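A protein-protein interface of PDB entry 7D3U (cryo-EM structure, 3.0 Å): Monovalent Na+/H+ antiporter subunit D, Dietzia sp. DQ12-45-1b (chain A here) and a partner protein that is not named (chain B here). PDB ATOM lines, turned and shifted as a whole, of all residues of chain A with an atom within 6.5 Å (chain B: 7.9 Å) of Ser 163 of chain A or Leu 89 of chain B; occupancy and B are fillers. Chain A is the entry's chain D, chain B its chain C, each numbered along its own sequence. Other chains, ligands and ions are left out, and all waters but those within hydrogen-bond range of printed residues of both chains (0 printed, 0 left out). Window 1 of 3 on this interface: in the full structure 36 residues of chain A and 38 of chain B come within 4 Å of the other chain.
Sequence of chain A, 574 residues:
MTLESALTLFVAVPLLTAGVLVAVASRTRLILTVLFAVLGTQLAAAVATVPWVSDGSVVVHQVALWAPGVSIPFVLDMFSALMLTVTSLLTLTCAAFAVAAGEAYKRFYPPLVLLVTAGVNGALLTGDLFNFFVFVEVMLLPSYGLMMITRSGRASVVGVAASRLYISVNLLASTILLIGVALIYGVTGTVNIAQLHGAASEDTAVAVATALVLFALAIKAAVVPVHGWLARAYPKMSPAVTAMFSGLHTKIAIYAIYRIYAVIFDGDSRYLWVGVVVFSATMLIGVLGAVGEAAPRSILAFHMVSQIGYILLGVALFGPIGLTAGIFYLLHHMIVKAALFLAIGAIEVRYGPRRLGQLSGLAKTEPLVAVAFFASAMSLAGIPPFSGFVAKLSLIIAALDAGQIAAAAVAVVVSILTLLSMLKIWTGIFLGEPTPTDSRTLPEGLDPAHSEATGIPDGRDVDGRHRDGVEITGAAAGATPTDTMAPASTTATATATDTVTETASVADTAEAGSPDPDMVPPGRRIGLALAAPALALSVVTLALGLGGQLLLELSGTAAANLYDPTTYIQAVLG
CG of Met 148 of chain A touches OH of Tyr 85 of chain B, 3.3 Å away.
Leu 89 of chain B touches Ser 163 of chain A (CD1 to OG, 3.4 Å).
Arg 164 of chain A touches Met 23 of chain B.
Ala 90 of chain B touches Arg 164 of chain A.
Ile 82 of chain B touches Ile 167 of chain A (CG2 to CG2, 3.8 Å).
Ile 167 of chain A touches Tyr 85 of chain B (CD1 to CE2, 3.4 Å).
Leu 86 of chain B touches Ile 167 of chain A (CD2 to CG2, 3.7 Å).
Ile 167 of chain A touches Leu 89 of chain B.
Ser 168 of chain A touches Met 23 of chain B.
No residue of chain B comes within 4 Å of Ala 162 of chain A.
Of the printed residues of chain A, Leu 86 of chain B touches Ile 167.
Printed residues of chain B within 4 Å of Ile 167 of chain A: Ile 82, Tyr 85, Leu 86 and Leu 89.
Printed residues of chain A within 4 Å of Ile 82 of chain B: Ile 167 (3.8 Å).
Ile 92 of chain B touches none of the printed residues of chain A.
Leu 87 of chain B touches none of the printed residues of chain A.
The nearest residue of chain B that does not touch Ser 163 of chain A is Tyr 85 of chain B (4.2 Å).
The nearest printed residue of chain A that does not touch Leu 89 of chain B is Val 160 of chain A (4.01 Å).
The nearest printed residue of chain A that does not touch Leu 86 of chain B is Ser 168 of chain A (4.5 Å).
O of Tyr 144 of chain A sits at hydrogen-bond distance from OH of Tyr 85 of chain B, 3.3 Å away.
O of Leu 89 of chain B sits at hydrogen-bond distance from NH2 of Arg 164 of chain A, at 3.2 Å.
NH2 of Arg 164 of chain A sits at hydrogen-bond distance from O of Gly 93 of chain B (3.4 Å).
Of the 17 printed residues of chain A, 6 touch a printed residue of chain B.
Printed residues of chain A that touch a printed residue of chain B: Tyr 144, Met 148, Ser 163, Arg 164, Ile 167 and Ser 168.
Of the 17 printed residues of chain B, 7 touch a printed residue of chain A.
Hydrophobic or aromatic side chains of chain B within 4 Å of the printed part of chain A: Met 23, Ile 82, Tyr 85, Leu 86 and Leu 89.
Among the printed residues, no Asp or Glu carboxylate lies within 4 Å of a Lys or Arg side-chain nitrogen of the other chain.
The backbone carbonyl oxygen of Arg 164 of chain A sits at hydrogen-bond distance from the side-chain hydroxyl of Ser 168 of chain A (3.0 Å).
The backbone NH (N) of Met 23 of chain B sits at hydrogen-bond distance from the backbone carbonyl oxygen (O) of Asp 97 of chain B (2.8 Å).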
ATOM      1  N   TYR A 144     -18.985   1.451 -15.350  1.00  0.00           N
ATOM      2  CA  TYR A 144     -20.300   0.963 -15.744  1.00  0.00           C
ATOM      3  C   TYR A 144     -20.533  -0.457 -15.253  1.00  0.00           C
ATOM      4  O   TYR A 144     -21.665  -0.817 -14.910  1.00  0.00           O
ATOM      5  CB  TYR A 144     -20.458   1.033 -17.261  1.00  0.00           C
ATOM      6  CG  TYR A 144     -20.166   2.393 -17.853  1.00  0.00           C
ATOM      7  CD1 TYR A 144     -20.320   3.550 -17.103  1.00  0.00           C
ATOM      8  CD2 TYR A 144     -19.738   2.519 -19.167  1.00  0.00           C
ATOM      9  CE1 TYR A 144     -20.054   4.790 -17.641  1.00  0.00           C
ATOM     10  CE2 TYR A 144     -19.470   3.756 -19.714  1.00  0.00           C
ATOM     11  CZ  TYR A 144     -19.630   4.887 -18.947  1.00  0.00           C
ATOM     12  OH  TYR A 144     -19.364   6.123 -19.488  1.00  0.00           O
ATOM     13  N   MET A 147     -21.449  -0.370 -11.533  1.00  0.00           N
ATOM     14  CA  MET A 147     -22.798   0.088 -11.229  1.00  0.00           C
ATOM     15  C   MET A 147     -23.801  -1.052 -11.160  1.00  0.00           C
ATOM     16  O   MET A 147     -24.905  -0.851 -10.644  1.00  0.00           O
ATOM     17  CB  MET A 147     -23.251   1.115 -12.265  1.00  0.00           C
ATOM     18  CG  MET A 147     -22.422   2.383 -12.272  1.00  0.00           C
ATOM     19  SD  MET A 147     -23.042   3.614 -13.426  1.00  0.00           S
ATOM     20  CE  MET A 147     -24.622   3.992 -12.680  1.00  0.00           C
ATOM     21  N   MET A 148     -23.450  -2.233 -11.666  1.00  0.00           N
ATOM     22  CA  MET A 148     -24.303  -3.406 -11.552  1.00  0.00           C
ATOM     23  C   MET A 148     -23.953  -4.282 -10.360  1.00  0.00           C
ATOM     24  O   MET A 148     -24.791  -5.081  -9.932  1.00  0.00           O
ATOM     25  CB  MET A 148     -24.226  -4.247 -12.831  1.00  0.00           C
ATOM     26  CG  MET A 148     -24.676  -3.517 -14.084  1.00  0.00           C
ATOM     27  SD  MET A 148     -26.433  -3.714 -14.424  1.00  0.00           S
ATOM     28  CE  MET A 148     -27.082  -2.216 -13.693  1.00  0.00           C
ATOM     29  N   VAL A 158     -34.566   0.614 -11.518  1.00  0.00           N
ATOM     30  CA  VAL A 158     -34.033   1.927 -11.179  1.00  0.00           C
ATOM     31  C   VAL A 158     -32.518   1.940 -11.318  1.00  0.00           C
ATOM     32  O   VAL A 158     -31.936   2.886 -11.864  1.00  0.00           O
ATOM     33  CB  VAL A 158     -34.473   2.324  -9.760  1.00  0.00           C
ATOM     34  CG1 VAL A 158     -33.915   3.680  -9.395  1.00  0.00           C
ATOM     35  CG2 VAL A 158     -35.980   2.318  -9.660  1.00  0.00           C
ATOM     36  N   GLY A 159     -31.855   0.901 -10.815  1.00  0.00           N
ATOM     37  CA  GLY A 159     -30.413   0.799 -10.924  1.00  0.00           C
ATOM     38  C   GLY A 159     -29.902   0.607 -12.333  1.00  0.00           C
ATOM     39  O   GLY A 159     -28.689   0.698 -12.549  1.00  0.00           O
ATOM     40  N   VAL A 160     -30.788   0.341 -13.291  1.00  0.00           N
ATOM     41  CA  VAL A 160     -30.378   0.179 -14.679  1.00  0.00           C
ATOM     42  C   VAL A 160     -30.766   1.432 -15.450  1.00  0.00           C
ATOM     43  O   VAL A 160     -30.099   1.804 -16.419  1.00  0.00           O
ATOM     44  CB  VAL A 160     -30.984  -1.090 -15.305  1.00  0.00           C
ATOM     45  CG1 VAL A 160     -30.652  -1.182 -16.774  1.00  0.00           C
ATOM     46  CG2 VAL A 160     -30.490  -2.319 -14.578  1.00  0.00           C
ATOM     47  N   ALA A 161     -31.823   2.117 -15.009  1.00  0.00           N
ATOM     48  CA  ALA A 161     -32.152   3.407 -15.606  1.00  0.00           C
ATOM     49  C   ALA A 161     -31.113   4.454 -15.234  1.00  0.00           C
ATOM     50  O   ALA A 161     -30.729   5.285 -16.068  1.00  0.00           O
ATOM     51  CB  ALA A 161     -33.546   3.850 -15.171  1.00  0.00           C
ATOM     52  N   ALA A 162     -30.640   4.424 -13.987  1.00  0.00           N
ATOM     53  CA  ALA A 162     -29.543   5.299 -13.593  1.00  0.00           C
ATOM     54  C   ALA A 162     -28.295   5.013 -14.413  1.00  0.00           C
ATOM     55  O   ALA A 162     -27.580   5.938 -14.810  1.00  0.00           O
ATOM     56  CB  ALA A 162     -29.251   5.141 -12.104  1.00  0.00           C
ATOM     57  N   SER A 163     -28.021   3.735 -14.687  1.00  0.00           N
ATOM     58  CA  SER A 163     -26.862   3.389 -15.501  1.00  0.00           C
ATOM     59  C   SER A 163     -27.037   3.860 -16.938  1.00  0.00           C
ATOM     60  O   SER A 163     -26.083   4.342 -17.560  1.00  0.00           O
ATOM     61  CB  SER A 163     -26.619   1.884 -15.453  1.00  0.00           C
ATOM     62  OG  SER A 163     -25.570   1.511 -16.327  1.00  0.00           O
ATOM     63  N   ARG A 164     -28.246   3.721 -17.485  1.00  0.00           N
ATOM     64  CA  ARG A 164     -28.531   4.255 -18.811  1.00  0.00           C
ATOM     65  C   ARG A 164     -28.242   5.746 -18.865  1.00  0.00           C
ATOM     66  O   ARG A 164     -27.551   6.223 -19.770  1.00  0.00           O
ATOM     67  CB  ARG A 164     -29.987   3.990 -19.193  1.00  0.00           C
ATOM     68  CG  ARG A 164     -30.300   2.571 -19.607  1.00  0.00           C
ATOM     69  CD  ARG A 164     -31.766   2.456 -19.982  1.00  0.00           C
ATOM     70  NE  ARG A 164     -32.205   1.073 -20.107  1.00  0.00           N
ATOM     71  CZ  ARG A 164     -33.460   0.712 -20.344  1.00  0.00           C
ATOM     72  NH1 ARG A 164     -34.401   1.636 -20.480  1.00  0.00           N
ATOM     73  NH2 ARG A 164     -33.777  -0.569 -20.444  1.00  0.00           N
ATOM     74  N   LEU A 165     -28.764   6.496 -17.893  1.00  0.00           N
ATOM     75  CA  LEU A 165     -28.551   7.941 -17.874  1.00  0.00           C
ATOM     76  C   LEU A 165     -27.072   8.281 -17.740  1.00  0.00           C
ATOM     77  O   LEU A 165     -26.560   9.164 -18.441  1.00  0.00           O
ATOM     78  CB  LEU A 165     -29.348   8.566 -16.733  1.00  0.00           C
ATOM     79  CG  LEU A 165     -29.019  10.016 -16.403  1.00  0.00           C
ATOM     80  CD1 LEU A 165     -29.332  10.898 -17.592  1.00  0.00           C
ATOM     81  CD2 LEU A 165     -29.790  10.463 -15.180  1.00  0.00           C
ATOM     82  N   TYR A 166     -26.373   7.585 -16.843  1.00  0.00           N
ATOM     83  CA  TYR A 166     -24.951   7.820 -16.625  1.00  0.00           C
ATOM     84  C   TYR A 166     -24.162   7.624 -17.911  1.00  0.00           C
ATOM     85  O   TYR A 166     -23.430   8.517 -18.352  1.00  0.00           O
ATOM     86  CB  TYR A 166     -24.448   6.876 -15.533  1.00  0.00           C
ATOM     87  CG  TYR A 166     -23.135   7.272 -14.912  1.00  0.00           C
ATOM     88  CD1 TYR A 166     -23.088   8.188 -13.876  1.00  0.00           C
ATOM     89  CD2 TYR A 166     -21.941   6.722 -15.355  1.00  0.00           C
ATOM     90  CE1 TYR A 166     -21.892   8.550 -13.300  1.00  0.00           C
ATOM     91  CE2 TYR A 166     -20.739   7.080 -14.787  1.00  0.00           C
ATOM     92  CZ  TYR A 166     -20.722   7.995 -13.759  1.00  0.00           C
ATOM     93  OH  TYR A 166     -19.532   8.362 -13.182  1.00  0.00           O
ATOM     94  N   ILE A 167     -24.303   6.451 -18.529  1.00  0.00           N
ATOM     95  CA  ILE A 167     -23.534   6.145 -19.732  1.00  0.00           C
ATOM     96  C   ILE A 167     -23.935   7.062 -20.877  1.00  0.00           C
ATOM     97  O   ILE A 167     -23.098   7.459 -21.694  1.00  0.00           O
ATOM     98  CB  ILE A 167     -23.705   4.663 -20.102  1.00  0.00           C
ATOM     99  CG1 ILE A 167     -23.290   3.792 -18.923  1.00  0.00           C
ATOM    100  CG2 ILE A 167     -22.874   4.317 -21.319  1.00  0.00           C
ATOM    101  CD1 ILE A 167     -23.806   2.399 -19.003  1.00  0.00           C
ATOM    102  N   SER A 168     -25.216   7.427 -20.952  1.00  0.00           N
ATOM    103  CA  SER A 168     -25.673   8.285 -22.037  1.00  0.00           C
ATOM    104  C   SER A 168     -25.047   9.668 -21.942  1.00  0.00           C
ATOM    105  O   SER A 168     -24.444  10.154 -22.905  1.00  0.00           O
ATOM    106  CB  SER A 168     -27.195   8.374 -22.021  1.00  0.00           C
ATOM    107  OG  SER A 168     -27.773   7.237 -22.637  1.00  0.00           O
ATOM    108  N   ARG A 232     -29.081  12.237 -10.232  1.00  0.00           N
ATOM    109  CA  ARG A 232     -30.024  11.162 -10.500  1.00  0.00           C
ATOM    110  C   ARG A 232     -29.341   9.867 -10.921  1.00  0.00           C
ATOM    111  O   ARG A 232     -30.005   8.981 -11.466  1.00  0.00           O
ATOM    112  CB  ARG A 232     -31.022  11.595 -11.574  1.00  0.00           C
ATOM    113  CG  ARG A 232     -31.762  12.876 -11.250  1.00  0.00           C
ATOM    114  CD  ARG A 232     -32.676  12.694 -10.056  1.00  0.00           C
ATOM    115  NE  ARG A 232     -33.666  11.650 -10.289  1.00  0.00           N
ATOM    116  CZ  ARG A 232     -34.546  11.243  -9.382  1.00  0.00           C
ATOM    117  NH1 ARG A 232     -35.412  10.285  -9.680  1.00  0.00           N
ATOM    118  NH2 ARG A 232     -34.562  11.794  -8.177  1.00  0.00           N
ATOM    119  N   ALA A 233     -28.036   9.736 -10.694  1.00  0.00           N
ATOM    120  CA  ALA A 233     -27.341   8.508 -11.054  1.00  0.00           C
ATOM    121  C   ALA A 233     -26.539   7.961  -9.881  1.00  0.00           C
ATOM    122  O   ALA A 233     -26.384   6.744  -9.745  1.00  0.00           O
ATOM    123  CB  ALA A 233     -26.425   8.738 -12.254  1.00  0.00           C
ATOM    124  N   LYS A 236     -28.780   6.087  -7.038  1.00  0.00           N
ATOM    125  CA  LYS A 236     -29.241   4.759  -7.436  1.00  0.00           C
ATOM    126  C   LYS A 236     -28.078   3.832  -7.772  1.00  0.00           C
ATOM    127  O   LYS A 236     -28.024   3.227  -8.840  1.00  0.00           O
ATOM    128  CB  LYS A 236     -30.202   4.884  -8.609  1.00  0.00           C
ATOM    129  CG  LYS A 236     -31.209   5.999  -8.433  1.00  0.00           C
ATOM    130  CD  LYS A 236     -31.737   6.493  -9.759  1.00  0.00           C
ATOM    131  CE  LYS A 236     -32.356   7.865  -9.601  1.00  0.00           C
ATOM    132  NZ  LYS A 236     -32.972   8.028  -8.258  1.00  0.00           N
ATOM    133  N   MET B  23     -34.808   3.254 -25.996  1.00  0.00           N
ATOM    134  CA  MET B  23     -33.372   3.213 -25.749  1.00  0.00           C
ATOM    135  C   MET B  23     -32.584   2.855 -27.000  1.00  0.00           C
ATOM    136  O   MET B  23     -31.456   3.330 -27.170  1.00  0.00           O
ATOM    137  CB  MET B  23     -33.052   2.225 -24.631  1.00  0.00           C
ATOM    138  CG  MET B  23     -31.643   2.360 -24.093  1.00  0.00           C
ATOM    139  SD  MET B  23     -31.332   4.006 -23.436  1.00  0.00           S
ATOM    140  CE  MET B  23     -29.556   3.956 -23.235  1.00  0.00           C
ATOM    141  N   ILE B  27     -29.507   4.754 -28.779  1.00  0.00           N
ATOM    142  CA  ILE B  27     -28.235   4.144 -29.143  1.00  0.00           C
ATOM    143  C   ILE B  27     -27.909   4.415 -30.604  1.00  0.00           C
ATOM    144  O   ILE B  27     -26.741   4.580 -30.967  1.00  0.00           O
ATOM    145  CB  ILE B  27     -28.268   2.637 -28.833  1.00  0.00           C
ATOM    146  CG1 ILE B  27     -28.371   2.419 -27.326  1.00  0.00           C
ATOM    147  CG2 ILE B  27     -27.033   1.945 -29.372  1.00  0.00           C
ATOM    148  CD1 ILE B  27     -28.814   1.034 -26.947  1.00  0.00           C
ATOM    149  N   ILE B  82     -18.736   0.861 -25.867  1.00  0.00           N
ATOM    150  CA  ILE B  82     -19.807   1.561 -25.165  1.00  0.00           C
ATOM    151  C   ILE B  82     -21.160   1.268 -25.803  1.00  0.00           C
ATOM    152  O   ILE B  82     -22.172   1.161 -25.104  1.00  0.00           O
ATOM    153  CB  ILE B  82     -19.524   3.072 -25.113  1.00  0.00           C
ATOM    154  CG1 ILE B  82     -18.124   3.327 -24.561  1.00  0.00           C
ATOM    155  CG2 ILE B  82     -20.551   3.772 -24.251  1.00  0.00           C
ATOM    156  CD1 ILE B  82     -17.814   4.786 -24.332  1.00  0.00           C
ATOM    157  N   THR B  83     -21.202   1.101 -27.127  1.00  0.00           N
ATOM    158  CA  THR B  83     -22.458   0.797 -27.799  1.00  0.00           C
ATOM    159  C   THR B  83     -22.929  -0.613 -27.473  1.00  0.00           C
ATOM    160  O   THR B  83     -24.125  -0.839 -27.267  1.00  0.00           O
ATOM    161  CB  THR B  83     -22.298   0.977 -29.308  1.00  0.00           C
ATOM    162  OG1 THR B  83     -22.205   2.372 -29.614  1.00  0.00           O
ATOM    163  CG2 THR B  83     -23.481   0.382 -30.053  1.00  0.00           C
ATOM    164  N   ILE B  84     -22.005  -1.574 -27.424  1.00  0.00           N
ATOM    165  CA  ILE B  84     -22.362  -2.925 -27.000  1.00  0.00           C
ATOM    166  C   ILE B  84     -22.978  -2.895 -25.608  1.00  0.00           C
ATOM    167  O   ILE B  84     -24.006  -3.536 -25.346  1.00  0.00           O
ATOM    168  CB  ILE B  84     -21.132  -3.849 -27.052  1.00  0.00           C
ATOM    169  CG1 ILE B  84     -20.667  -4.038 -28.493  1.00  0.00           C
ATOM    170  CG2 ILE B  84     -21.442  -5.193 -26.416  1.00  0.00           C
ATOM    171  CD1 ILE B  84     -19.321  -4.709 -28.604  1.00  0.00           C
ATOM    172  N   TYR B  85     -22.363  -2.142 -24.691  1.00  0.00           N
ATOM    173  CA  TYR B  85     -22.899  -2.124 -23.334  1.00  0.00           C
ATOM    174  C   TYR B  85     -24.237  -1.395 -23.269  1.00  0.00           C
ATOM    175  O   TYR B  85     -25.125  -1.787 -22.505  1.00  0.00           O
ATOM    176  CB  TYR B  85     -21.909  -1.510 -22.352  1.00  0.00           C
ATOM    177  CG  TYR B  85     -22.335  -1.753 -20.925  1.00  0.00           C
ATOM    178  CD1 TYR B  85     -22.185  -3.001 -20.342  1.00  0.00           C
ATOM    179  CD2 TYR B  85     -22.913  -0.747 -20.172  1.00  0.00           C
ATOM    180  CE1 TYR B  85     -22.589  -3.235 -19.043  1.00  0.00           C
ATOM    181  CE2 TYR B  85     -23.316  -0.973 -18.870  1.00  0.00           C
ATOM    182  CZ  TYR B  85     -23.151  -2.217 -18.311  1.00  0.00           C
ATOM    183  OH  TYR B  85     -23.551  -2.442 -17.017  1.00  0.00           O
ATOM    184  N   LEU B  86     -24.418  -0.344 -24.069  1.00  0.00           N
ATOM    185  CA  LEU B  86     -25.715   0.323 -24.093  1.00  0.00           C
ATOM    186  C   LEU B  86     -26.793  -0.599 -24.648  1.00  0.00           C
ATOM    187  O   LEU B  86     -27.929  -0.611 -24.156  1.00  0.00           O
ATOM    188  CB  LEU B  86     -25.629   1.608 -24.913  1.00  0.00           C
ATOM    189  CG  LEU B  86     -25.124   2.839 -24.161  1.00  0.00           C
ATOM    190  CD1 LEU B  86     -25.084   4.048 -25.078  1.00  0.00           C
ATOM    191  CD2 LEU B  86     -25.993   3.111 -22.951  1.00  0.00           C
ATOM    192  N   LEU B  87     -26.449  -1.397 -25.660  1.00  0.00           N
ATOM    193  CA  LEU B  87     -27.419  -2.319 -26.238  1.00  0.00           C
ATOM    194  C   LEU B  87     -27.799  -3.411 -25.250  1.00  0.00           C
ATOM    195  O   LEU B  87     -28.973  -3.783 -25.155  1.00  0.00           O
ATOM    196  CB  LEU B  87     -26.865  -2.925 -27.524  1.00  0.00           C
ATOM    197  CG  LEU B  87     -26.790  -1.964 -28.707  1.00  0.00           C
ATOM    198  CD1 LEU B  87     -25.831  -2.490 -29.752  1.00  0.00           C
ATOM    199  CD2 LEU B  87     -28.166  -1.739 -29.301  1.00  0.00           C
ATOM    200  N   VAL B  88     -26.825  -3.942 -24.507  1.00  0.00           N
ATOM    201  CA  VAL B  88     -27.182  -4.937 -23.502  1.00  0.00           C
ATOM    202  C   VAL B  88     -27.922  -4.288 -22.337  1.00  0.00           C
ATOM    203  O   VAL B  88     -28.677  -4.965 -21.631  1.00  0.00           O
ATOM    204  CB  VAL B  88     -25.943  -5.715 -23.015  1.00  0.00           C
ATOM    205  CG1 VAL B  88     -24.988  -4.811 -22.291  1.00  0.00           C
ATOM    206  CG2 VAL B  88     -26.347  -6.883 -22.141  1.00  0.00           C
ATOM    207  N   LEU B  89     -27.745  -2.979 -22.128  1.00  0.00           N
ATOM    208  CA  LEU B  89     -28.572  -2.268 -21.160  1.00  0.00           C
ATOM    209  C   LEU B  89     -30.001  -2.110 -21.654  1.00  0.00           C
ATOM    210  O   LEU B  89     -30.929  -2.008 -20.845  1.00  0.00           O
ATOM    211  CB  LEU B  89     -27.987  -0.886 -20.870  1.00  0.00           C
ATOM    212  CG  LEU B  89     -26.939  -0.707 -19.777  1.00  0.00           C
ATOM    213  CD1 LEU B  89     -26.999   0.713 -19.258  1.00  0.00           C
ATOM    214  CD2 LEU B  89     -27.141  -1.694 -18.651  1.00  0.00           C
ATOM    215  N   ALA B  90     -30.196  -2.074 -22.973  1.00  0.00           N
ATOM    216  CA  ALA B  90     -31.525  -1.830 -23.520  1.00  0.00           C
ATOM    217  C   ALA B  90     -32.483  -2.996 -23.311  1.00  0.00           C
ATOM    218  O   ALA B  90     -33.697  -2.801 -23.425  1.00  0.00           O
ATOM    219  CB  ALA B  90     -31.426  -1.511 -25.011  1.00  0.00           C
ATOM    220  N   VAL B  91     -31.984  -4.192 -23.008  1.00  0.00           N
ATOM    221  CA  VAL B  91     -32.830  -5.378 -22.978  1.00  0.00           C
ATOM    222  C   VAL B  91     -32.901  -5.999 -21.586  1.00  0.00           C
ATOM    223  O   VAL B  91     -33.211  -7.176 -21.454  1.00  0.00           O
ATOM    224  CB  VAL B  91     -32.364  -6.415 -24.017  1.00  0.00           C
ATOM    225  CG1 VAL B  91     -32.499  -5.851 -25.412  1.00  0.00           C
ATOM    226  CG2 VAL B  91     -30.933  -6.836 -23.740  1.00  0.00           C
ATOM    227  N   ILE B  92     -32.620  -5.229 -20.536  1.00  0.00           N
ATOM    228  CA  ILE B  92     -32.746  -5.709 -19.168  1.00  0.00           C
ATOM    229  C   ILE B  92     -33.730  -4.877 -18.358  1.00  0.00           C
ATOM    230  O   ILE B  92     -34.533  -5.427 -17.598  1.00  0.00           O
ATOM    231  CB  ILE B  92     -31.375  -5.772 -18.460  1.00  0.00           C
ATOM    232  CG1 ILE B  92     -30.473  -6.820 -19.101  1.00  0.00           C
ATOM    233  CG2 ILE B  92     -31.558  -6.078 -16.989  1.00  0.00           C
ATOM    234  CD1 ILE B  92     -29.045  -6.737 -18.623  1.00  0.00           C
ATOM    235  N   GLY B  93     -33.693  -3.556 -18.502  1.00  0.00           N
ATOM    236  CA  GLY B  93     -34.605  -2.711 -17.748  1.00  0.00           C
ATOM    237  C   GLY B  93     -36.020  -2.810 -18.285  1.00  0.00           C
ATOM    238  O   GLY B  93     -36.246  -2.748 -19.499  1.00  0.00           O
ATOM    239  N   GLY B  94     -36.982  -2.958 -17.378  1.00  0.00           N
ATOM    240  CA  GLY B  94     -38.379  -3.052 -17.748  1.00  0.00           C
ATOM    241  C   GLY B  94     -38.667  -4.244 -18.650  1.00  0.00           C
ATOM    242  O   GLY B  94     -37.876  -5.172 -18.799  1.00  0.00           O
ATOM    243  N   ASP B  96     -39.713  -3.380 -21.827  1.00  0.00           N
ATOM    244  CA  ASP B  96     -39.476  -2.780 -23.131  1.00  0.00           C
ATOM    245  C   ASP B  96     -38.177  -1.988 -23.048  1.00  0.00           C
ATOM    246  O   ASP B  96     -37.424  -2.091 -22.076  1.00  0.00           O
ATOM    247  CB  ASP B  96     -40.659  -1.900 -23.551  1.00  0.00           C
ATOM    248  CG  ASP B  96     -41.885  -2.707 -23.904  1.00  0.00           C
ATOM    249  OD1 ASP B  96     -41.748  -3.931 -24.099  1.00  0.00           O
ATOM    250  OD2 ASP B  96     -42.984  -2.120 -23.983  1.00  0.00           O
ATOM    251  N   ASP B  97     -37.908  -1.193 -24.080  1.00  0.00           N
ATOM    252  CA  ASP B  97     -36.801  -0.248 -24.058  1.00  0.00           C
ATOM    253  C   ASP B  97     -37.284   1.187 -23.915  1.00  0.00           C
ATOM    254  O   ASP B  97     -36.506   2.119 -24.137  1.00  0.00           O
ATOM    255  CB  ASP B  97     -35.944  -0.402 -25.315  1.00  0.00           C
ATOM    256  CG  ASP B  97     -36.717  -0.129 -26.585  1.00  0.00           C
ATOM    257  OD1 ASP B  97     -37.940   0.106 -26.499  1.00  0.00           O
ATOM    258  OD2 ASP B  97     -36.100  -0.148 -27.669  1.00  0.00           O
